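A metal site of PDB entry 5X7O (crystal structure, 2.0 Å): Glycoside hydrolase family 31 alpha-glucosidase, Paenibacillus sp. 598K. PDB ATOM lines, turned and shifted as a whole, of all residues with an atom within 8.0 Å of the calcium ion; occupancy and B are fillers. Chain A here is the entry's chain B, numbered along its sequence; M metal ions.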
ATOM      1  N   THR A 562      22.171 -32.236  12.672  1.00  0.00           N
ATOM      2  CA  THR A 562      22.199 -31.562  11.388  1.00  0.00           C
ATOM      3  C   THR A 562      23.560 -30.916  11.157  1.00  0.00           C
ATOM      4  O   THR A 562      24.164 -31.081  10.089  1.00  0.00           O
ATOM      5  CB  THR A 562      21.105 -30.514  11.260  1.00  0.00           C
ATOM      6  OG1 THR A 562      19.848 -31.123  11.543  1.00  0.00           O
ATOM      7  CG2 THR A 562      21.074 -29.946   9.856  1.00  0.00           C
ATOM      8  N   ASP A 666      14.496 -26.682   6.424  1.00  0.00           N
ATOM      9  CA  ASP A 666      14.324 -27.698   7.454  1.00  0.00           C
ATOM     10  C   ASP A 666      15.566 -28.622   7.546  1.00  0.00           C
ATOM     11  O   ASP A 666      15.973 -28.985   8.650  1.00  0.00           O
ATOM     12  CB  ASP A 666      13.042 -28.489   7.198  1.00  0.00           C
ATOM     13  CG  ASP A 666      12.728 -29.472   8.326  1.00  0.00           C
ATOM     14  OD1 ASP A 666      12.907 -29.108   9.517  1.00  0.00           O
ATOM     15  OD2 ASP A 666      12.360 -30.618   8.024  1.00  0.00           O
ATOM     16  N   ASN A1114       4.824 -29.006  15.656  1.00  0.00           N
ATOM     17  CA  ASN A1114       6.079 -28.550  16.326  1.00  0.00           C
ATOM     18  C   ASN A1114       6.737 -29.626  17.186  1.00  0.00           C
ATOM     19  O   ASN A1114       7.299 -29.333  18.246  1.00  0.00           O
ATOM     20  CB  ASN A1114       5.816 -27.275  17.173  1.00  0.00           C
ATOM     21  CG  ASN A1114       7.089 -26.476  17.486  1.00  0.00           C
ATOM     22  OD1 ASN A1114       8.022 -26.433  16.669  1.00  0.00           O
ATOM     23  ND2 ASN A1114       7.145 -25.840  18.669  1.00  0.00           N
ATOM     24  N   GLY A1115       6.678 -30.874  16.722  1.00  0.00           N
ATOM     25  CA  GLY A1115       7.282 -32.006  17.443  1.00  0.00           C
ATOM     26  C   GLY A1115       8.784 -31.888  17.583  1.00  0.00           C
ATOM     27  O   GLY A1115       9.389 -32.491  18.464  1.00  0.00           O
ATOM     28  N   ASP A1116       9.395 -31.118  16.690  1.00  0.00           N
ATOM     29  CA  ASP A1116      10.849 -30.883  16.710  1.00  0.00           C
ATOM     30  C   ASP A1116      11.242 -29.558  17.407  1.00  0.00           C
ATOM     31  O   ASP A1116      12.431 -29.205  17.464  1.00  0.00           O
ATOM     32  CB  ASP A1116      11.387 -30.925  15.266  1.00  0.00           C
ATOM     33  CG  ASP A1116      10.713 -29.930  14.327  1.00  0.00           C
ATOM     34  OD1 ASP A1116       9.945 -29.018  14.786  1.00  0.00           O
ATOM     35  OD2 ASP A1116      10.944 -30.068  13.090  1.00  0.00           O
ATOM     36  N   PHE A1117      10.249 -28.817  17.901  1.00  0.00           N
ATOM     37  CA  PHE A1117      10.468 -27.559  18.612  1.00  0.00           C
ATOM     38  C   PHE A1117      11.256 -26.522  17.787  1.00  0.00           C
ATOM     39  O   PHE A1117      11.932 -25.675  18.347  1.00  0.00           O
ATOM     40  CB  PHE A1117      11.139 -27.807  19.970  1.00  0.00           C
ATOM     41  CG  PHE A1117      10.414 -28.801  20.823  1.00  0.00           C
ATOM     42  CD1 PHE A1117       9.247 -28.452  21.488  1.00  0.00           C
ATOM     43  CD2 PHE A1117      10.872 -30.096  20.929  1.00  0.00           C
ATOM     44  CE1 PHE A1117       8.554 -29.379  22.262  1.00  0.00           C
ATOM     45  CE2 PHE A1117      10.193 -31.035  21.720  1.00  0.00           C
ATOM     46  CZ  PHE A1117       9.037 -30.666  22.375  1.00  0.00           C
ATOM     47  N   GLU A1118      11.108 -26.569  16.472  1.00  0.00           N
ATOM     48  CA  GLU A1118      11.855 -25.688  15.576  1.00  0.00           C
ATOM     49  C   GLU A1118      11.168 -24.368  15.333  1.00  0.00           C
ATOM     50  O   GLU A1118      11.805 -23.427  14.842  1.00  0.00           O
ATOM     51  CB  GLU A1118      12.149 -26.388  14.258  1.00  0.00           C
ATOM     52  CG  GLU A1118      13.121 -27.544  14.423  1.00  0.00           C
ATOM     53  CD  GLU A1118      14.470 -27.079  14.956  1.00  0.00           C
ATOM     54  OE1 GLU A1118      15.001 -26.031  14.462  1.00  0.00           O
ATOM     55  OE2 GLU A1118      15.018 -27.756  15.848  1.00  0.00           O
ATOM     56  N   ARG A1119       9.898 -24.253  15.697  1.00  0.00           N
ATOM     57  CA  ARG A1119       9.197 -22.996  15.490  1.00  0.00           C
ATOM     58  C   ARG A1119       9.877 -21.857  16.285  1.00  0.00           C
ATOM     59  O   ARG A1119      10.389 -22.057  17.387  1.00  0.00           O
ATOM     60  CB  ARG A1119       7.733 -23.118  15.900  1.00  0.00           C
ATOM     61  CG  ARG A1119       6.874 -21.945  15.466  1.00  0.00           C
ATOM     62  CD  ARG A1119       5.397 -22.295  15.546  1.00  0.00           C
ATOM     63  NE  ARG A1119       5.141 -23.475  14.713  1.00  0.00           N
ATOM     64  CZ  ARG A1119       4.184 -24.383  14.911  1.00  0.00           C
ATOM     65  NH1 ARG A1119       3.325 -24.283  15.923  1.00  0.00           N
ATOM     66  NH2 ARG A1119       4.098 -25.417  14.083  1.00  0.00           N
ATOM     67  N   ILE A1141      12.326 -23.633  25.495  1.00  0.00           N
ATOM     68  CA  ILE A1141      12.845 -24.091  24.212  1.00  0.00           C
ATOM     69  C   ILE A1141      13.954 -23.113  23.820  1.00  0.00           C
ATOM     70  O   ILE A1141      13.693 -21.921  23.778  1.00  0.00           O
ATOM     71  CB  ILE A1141      11.762 -24.060  23.127  1.00  0.00           C
ATOM     72  CG1 ILE A1141      10.626 -25.044  23.452  1.00  0.00           C
ATOM     73  CG2 ILE A1141      12.354 -24.410  21.764  1.00  0.00           C
ATOM     74  CD1 ILE A1141       9.344 -24.754  22.691  1.00  0.00           C
ATOM     75  N   ASP A1142      15.145 -23.627  23.564  1.00  0.00           N
ATOM     76  CA  ASP A1142      16.208 -22.848  22.909  1.00  0.00           C
ATOM     77  C   ASP A1142      17.239 -23.782  22.230  1.00  0.00           C
ATOM     78  O   ASP A1142      16.963 -24.971  22.087  1.00  0.00           O
ATOM     79  CB  ASP A1142      16.839 -21.841  23.894  1.00  0.00           C
ATOM     80  CG  ASP A1142      17.555 -22.503  25.053  1.00  0.00           C
ATOM     81  OD1 ASP A1142      18.215 -23.555  24.870  1.00  0.00           O
ATOM     82  OD2 ASP A1142      17.469 -21.945  26.169  1.00  0.00           O
ATOM     83  N   GLY A1152      23.511 -29.074  22.620  1.00  0.00           N
ATOM     84  CA  GLY A1152      22.728 -28.715  21.448  1.00  0.00           C
ATOM     85  C   GLY A1152      21.446 -29.515  21.258  1.00  0.00           C
ATOM     86  O   GLY A1152      21.067 -30.321  22.121  1.00  0.00           O
ATOM     87  N   PRO A1153      20.773 -29.317  20.106  1.00  0.00           N
ATOM     88  CA  PRO A1153      19.586 -30.108  19.780  1.00  0.00           C
ATOM     89  C   PRO A1153      19.944 -31.483  19.286  1.00  0.00           C
ATOM     90  O   PRO A1153      21.107 -31.740  18.994  1.00  0.00           O
ATOM     91  CB  PRO A1153      18.912 -29.290  18.662  1.00  0.00           C
ATOM     92  CG  PRO A1153      19.748 -28.073  18.466  1.00  0.00           C
ATOM     93  CD  PRO A1153      21.098 -28.367  19.031  1.00  0.00           C
ATOM     94  N   ALA A1154      18.951 -32.365  19.161  1.00  0.00           N
ATOM     95  CA  ALA A1154      19.160 -33.661  18.480  1.00  0.00           C
ATOM     96  C   ALA A1154      19.191 -33.433  16.962  1.00  0.00           C
ATOM     97  O   ALA A1154      19.945 -34.085  16.268  1.00  0.00           O
ATOM     98  CB  ALA A1154      18.089 -34.670  18.848  1.00  0.00           C
ATOM     99  N   ARG A1155      18.388 -32.484  16.475  1.00  0.00           N
ATOM    100  CA  ARG A1155      18.350 -32.133  15.048  1.00  0.00           C
ATOM    101  C   ARG A1155      18.002 -30.666  14.858  1.00  0.00           C
ATOM    102  O   ARG A1155      17.217 -30.088  15.607  1.00  0.00           O
ATOM    103  CB  ARG A1155      17.332 -33.004  14.287  1.00  0.00           C
ATOM    104  CG  ARG A1155      17.497 -33.022  12.762  1.00  0.00           C
ATOM    105  CD  ARG A1155      16.303 -33.638  12.038  1.00  0.00           C
ATOM    106  NE  ARG A1155      15.144 -32.755  12.108  1.00  0.00           N
ATOM    107  CZ  ARG A1155      14.944 -31.695  11.316  1.00  0.00           C
ATOM    108  NH1 ARG A1155      15.798 -31.350  10.351  1.00  0.00           N
ATOM    109  NH2 ARG A1155      13.845 -30.961  11.499  1.00  0.00           N
ATOM    110  N   ARG A1156      18.572 -30.064  13.816  1.00  0.00           N
ATOM    111  CA  ARG A1156      18.324 -28.676  13.446  1.00  0.00           C
ATOM    112  C   ARG A1156      18.720 -27.709  14.590  1.00  0.00           C
ATOM    113  O   ARG A1156      19.826 -27.845  15.098  1.00  0.00           O
ATOM    114  CB  ARG A1156      16.920 -28.507  12.878  1.00  0.00           C
ATOM    115  CG  ARG A1156      16.796 -27.316  11.940  1.00  0.00           C
ATOM    116  CD  ARG A1156      15.421 -27.174  11.321  1.00  0.00           C
ATOM    117  NE  ARG A1156      15.332 -25.974  10.499  1.00  0.00           N
ATOM    118  CZ  ARG A1156      15.124 -24.745  10.962  1.00  0.00           C
ATOM    119  NH1 ARG A1156      14.962 -24.509  12.262  1.00  0.00           N
ATOM    120  NH2 ARG A1156      15.080 -23.730  10.118  1.00  0.00           N
ATOM    121  N   ASN A1157      17.881 -26.749  14.973  1.00  0.00           N
ATOM    122  CA  ASN A1157      18.344 -25.583  15.726  1.00  0.00           C
ATOM    123  C   ASN A1157      17.935 -25.530  17.187  1.00  0.00           C
ATOM    124  O   ASN A1157      18.601 -24.868  17.962  1.00  0.00           O
ATOM    125  CB  ASN A1157      17.863 -24.294  15.056  1.00  0.00           C
ATOM    126  CG  ASN A1157      18.817 -23.134  15.249  1.00  0.00           C
ATOM    127  OD1 ASN A1157      20.028 -23.320  15.333  1.00  0.00           O
ATOM    128  ND2 ASN A1157      18.281 -21.925  15.280  1.00  0.00           N
ATOM    129  N   GLN A1158      16.864 -26.232  17.561  1.00  0.00           N
ATOM    130  CA  GLN A1158      16.221 -26.043  18.862  1.00  0.00           C
ATOM    131  C   GLN A1158      15.795 -27.362  19.493  1.00  0.00           C
ATOM    132  O   GLN A1158      15.538 -28.349  18.796  1.00  0.00           O
ATOM    133  CB  GLN A1158      15.036 -25.094  18.701  1.00  0.00           C
ATOM    134  CG  GLN A1158      15.445 -23.634  18.612  1.00  0.00           C
ATOM    135  CD  GLN A1158      14.276 -22.653  18.442  1.00  0.00           C
ATOM    136  OE1 GLN A1158      14.497 -21.455  18.491  1.00  0.00           O
ATOM    137  NE2 GLN A1158      13.045 -23.167  18.261  1.00  0.00           N
ATOM    138  N   ARG A1159      15.741 -27.381  20.809  1.00  0.00           N
ATOM    139  CA  ARG A1159      15.188 -28.504  21.559  1.00  0.00           C
ATOM    140  C   ARG A1159      14.502 -27.973  22.817  1.00  0.00           C
ATOM    141  O   ARG A1159      14.857 -26.911  23.316  1.00  0.00           O
ATOM    142  CB  ARG A1159      16.274 -29.527  21.887  1.00  0.00           C
ATOM    143  CG  ARG A1159      17.209 -29.186  23.037  1.00  0.00           C
ATOM    144  CD  ARG A1159      18.238 -28.093  22.678  1.00  0.00           C
ATOM    145  NE  ARG A1159      19.195 -27.873  23.760  1.00  0.00           N
ATOM    146  CZ  ARG A1159      19.003 -27.090  24.827  1.00  0.00           C
ATOM    147  NH1 ARG A1159      17.851 -26.438  25.010  1.00  0.00           N
ATOM    148  NH2 ARG A1159      19.971 -26.954  25.730  1.00  0.00           N
ATOM    149  N   ALA A1160      13.500 -28.704  23.307  1.00  0.00           N
ATOM    150  CA  ALA A1160      12.838 -28.369  24.549  1.00  0.00           C
ATOM    151  C   ALA A1160      13.709 -28.829  25.701  1.00  0.00           C
ATOM    152  O   ALA A1160      14.548 -29.739  25.549  1.00  0.00           O
ATOM    153  CB  ALA A1160      11.469 -29.031  24.623  1.00  0.00           C
ATOM    154  N   TRP A1223      22.102 -38.160  24.068  1.00  0.00           N
ATOM    155  CA  TRP A1223      20.880 -38.330  23.300  1.00  0.00           C
ATOM    156  C   TRP A1223      20.550 -39.818  23.119  1.00  0.00           C
ATOM    157  O   TRP A1223      21.425 -40.599  22.774  1.00  0.00           O
ATOM    158  CB  TRP A1223      20.966 -37.647  21.930  1.00  0.00           C
ATOM    159  CG  TRP A1223      20.800 -36.175  21.964  1.00  0.00           C
ATOM    160  CD1 TRP A1223      21.742 -35.237  21.646  1.00  0.00           C
ATOM    161  CD2 TRP A1223      19.615 -35.447  22.333  1.00  0.00           C
ATOM    162  NE1 TRP A1223      21.219 -33.977  21.799  1.00  0.00           N
ATOM    163  CE2 TRP A1223      19.919 -34.076  22.224  1.00  0.00           C
ATOM    164  CE3 TRP A1223      18.332 -35.827  22.749  1.00  0.00           C
ATOM    165  CZ2 TRP A1223      18.989 -33.089  22.491  1.00  0.00           C
ATOM    166  CZ3 TRP A1223      17.403 -34.847  23.023  1.00  0.00           C
ATOM    167  CH2 TRP A1223      17.730 -33.489  22.897  1.00  0.00           C
ATOM    168  N   ILE A1254      14.462 -32.656  25.222  1.00  0.00           N
ATOM    169  CA  ILE A1254      13.518 -33.377  24.415  1.00  0.00           C
ATOM    170  C   ILE A1254      13.544 -32.794  23.009  1.00  0.00           C
ATOM    171  O   ILE A1254      13.474 -31.574  22.845  1.00  0.00           O
ATOM    172  CB  ILE A1254      12.072 -33.252  24.946  1.00  0.00           C
ATOM    173  CG1 ILE A1254      11.973 -33.702  26.423  1.00  0.00           C
ATOM    174  CG2 ILE A1254      11.128 -34.096  24.102  1.00  0.00           C
ATOM    175  CD1 ILE A1254      10.728 -33.209  27.109  1.00  0.00           C
ATOM    176  N   ASP A1255      13.639 -33.663  22.003  1.00  0.00           N
ATOM    177  CA  ASP A1255      13.638 -33.256  20.608  1.00  0.00           C
ATOM    178  C   ASP A1255      13.028 -34.306  19.648  1.00  0.00           C
ATOM    179  O   ASP A1255      12.879 -35.475  19.983  1.00  0.00           O
ATOM    180  CB  ASP A1255      15.079 -32.894  20.188  1.00  0.00           C
ATOM    181  CG  ASP A1255      15.136 -31.889  19.060  1.00  0.00           C
ATOM    182  OD1 ASP A1255      14.061 -31.450  18.614  1.00  0.00           O
ATOM    183  OD2 ASP A1255      16.232 -31.519  18.587  1.00  0.00           O
ATOM    184  N   GLU A1256      12.663 -33.848  18.450  1.00  0.00           N
ATOM    185  CA  GLU A1256      12.293 -34.728  17.346  1.00  0.00           C
ATOM    186  C   GLU A1256      11.199 -35.740  17.744  1.00  0.00           C
ATOM    187  O   GLU A1256      11.321 -36.961  17.515  1.00  0.00           O
ATOM    188  CB  GLU A1256      13.538 -35.414  16.758  1.00  0.00           C
ATOM    189  CG  GLU A1256      14.654 -34.458  16.309  1.00  0.00           C
ATOM    190  CD  GLU A1256      14.166 -33.307  15.415  1.00  0.00           C
ATOM    191  OE1 GLU A1256      13.580 -33.571  14.359  1.00  0.00           O
ATOM    192  OE2 GLU A1256      14.383 -32.124  15.757  1.00  0.00           O
ATOM    193  N   VAL A1257      10.127 -35.214  18.315  1.00  0.00           N
ATOM    194  CA  VAL A1257       8.992 -36.026  18.735  1.00  0.00           C
ATOM    195  C   VAL A1257       8.130 -36.252  17.499  1.00  0.00           C
ATOM    196  O   VAL A1257       7.739 -35.271  16.831  1.00  0.00           O
ATOM    197  CB  VAL A1257       8.130 -35.336  19.824  1.00  0.00           C
ATOM    198  CG1 VAL A1257       7.150 -36.325  20.456  1.00  0.00           C
ATOM    199  CG2 VAL A1257       8.996 -34.743  20.921  1.00  0.00           C
HETATM  200 CA    CA M   1      14.830 -29.790  17.118  1.00  0.00          CA
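The calcium ion is bound by O of Gln 1158 (2.3 Å), OD1 of Asp 1255 (2.4 Å), OE2 of Glu 1118 (2.4 Å), O of Asp 1116 (2.5 Å), OD2 of Asp 1255 (2.7 Å), OE2 of Glu 1256 (2.7 Å) and O of Arg 1155 (2.8 Å).
The calcium ion has seven donor atoms within binding distance.
The guanidinium group (NH2) of Arg 1155 is in salt-bridge range of the side-chain carboxylate (OD1) of Asp 666, at 2.9 Å.
The side-chain carboxylate of Asp 1255 sits close to the backbone NH of Ala 1154.
OE1 of Glu 1118 is in salt-bridge range of NH1 of Arg 1156, at 2.7 Å.
The backbone NH (N) of Glu 1118 is in hydrogen-bond range of the side-chain amide oxygen (OD1) of Asn 1114.
The backbone NH (N) of Asn 1157 lies within hydrogen-bond range of the side-chain carboxylate (OE1) of Glu 1118 (3.0 Å).
O of Arg 1119 lies within hydrogen-bond range of NE2 of Gln 1158, 3.0 Å away.
The side-chain amide nitrogen (NE2) of Gln 1158 is in hydrogen-bond range of the backbone carbonyl oxygen (O) of Phe 1117.
Along chain A the residues within 4 Å of the calcium ion span positions 1116 to 1256.
The nearest printed residue that does not touch the calcium ion is Pro 1153 (4.4 Å).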
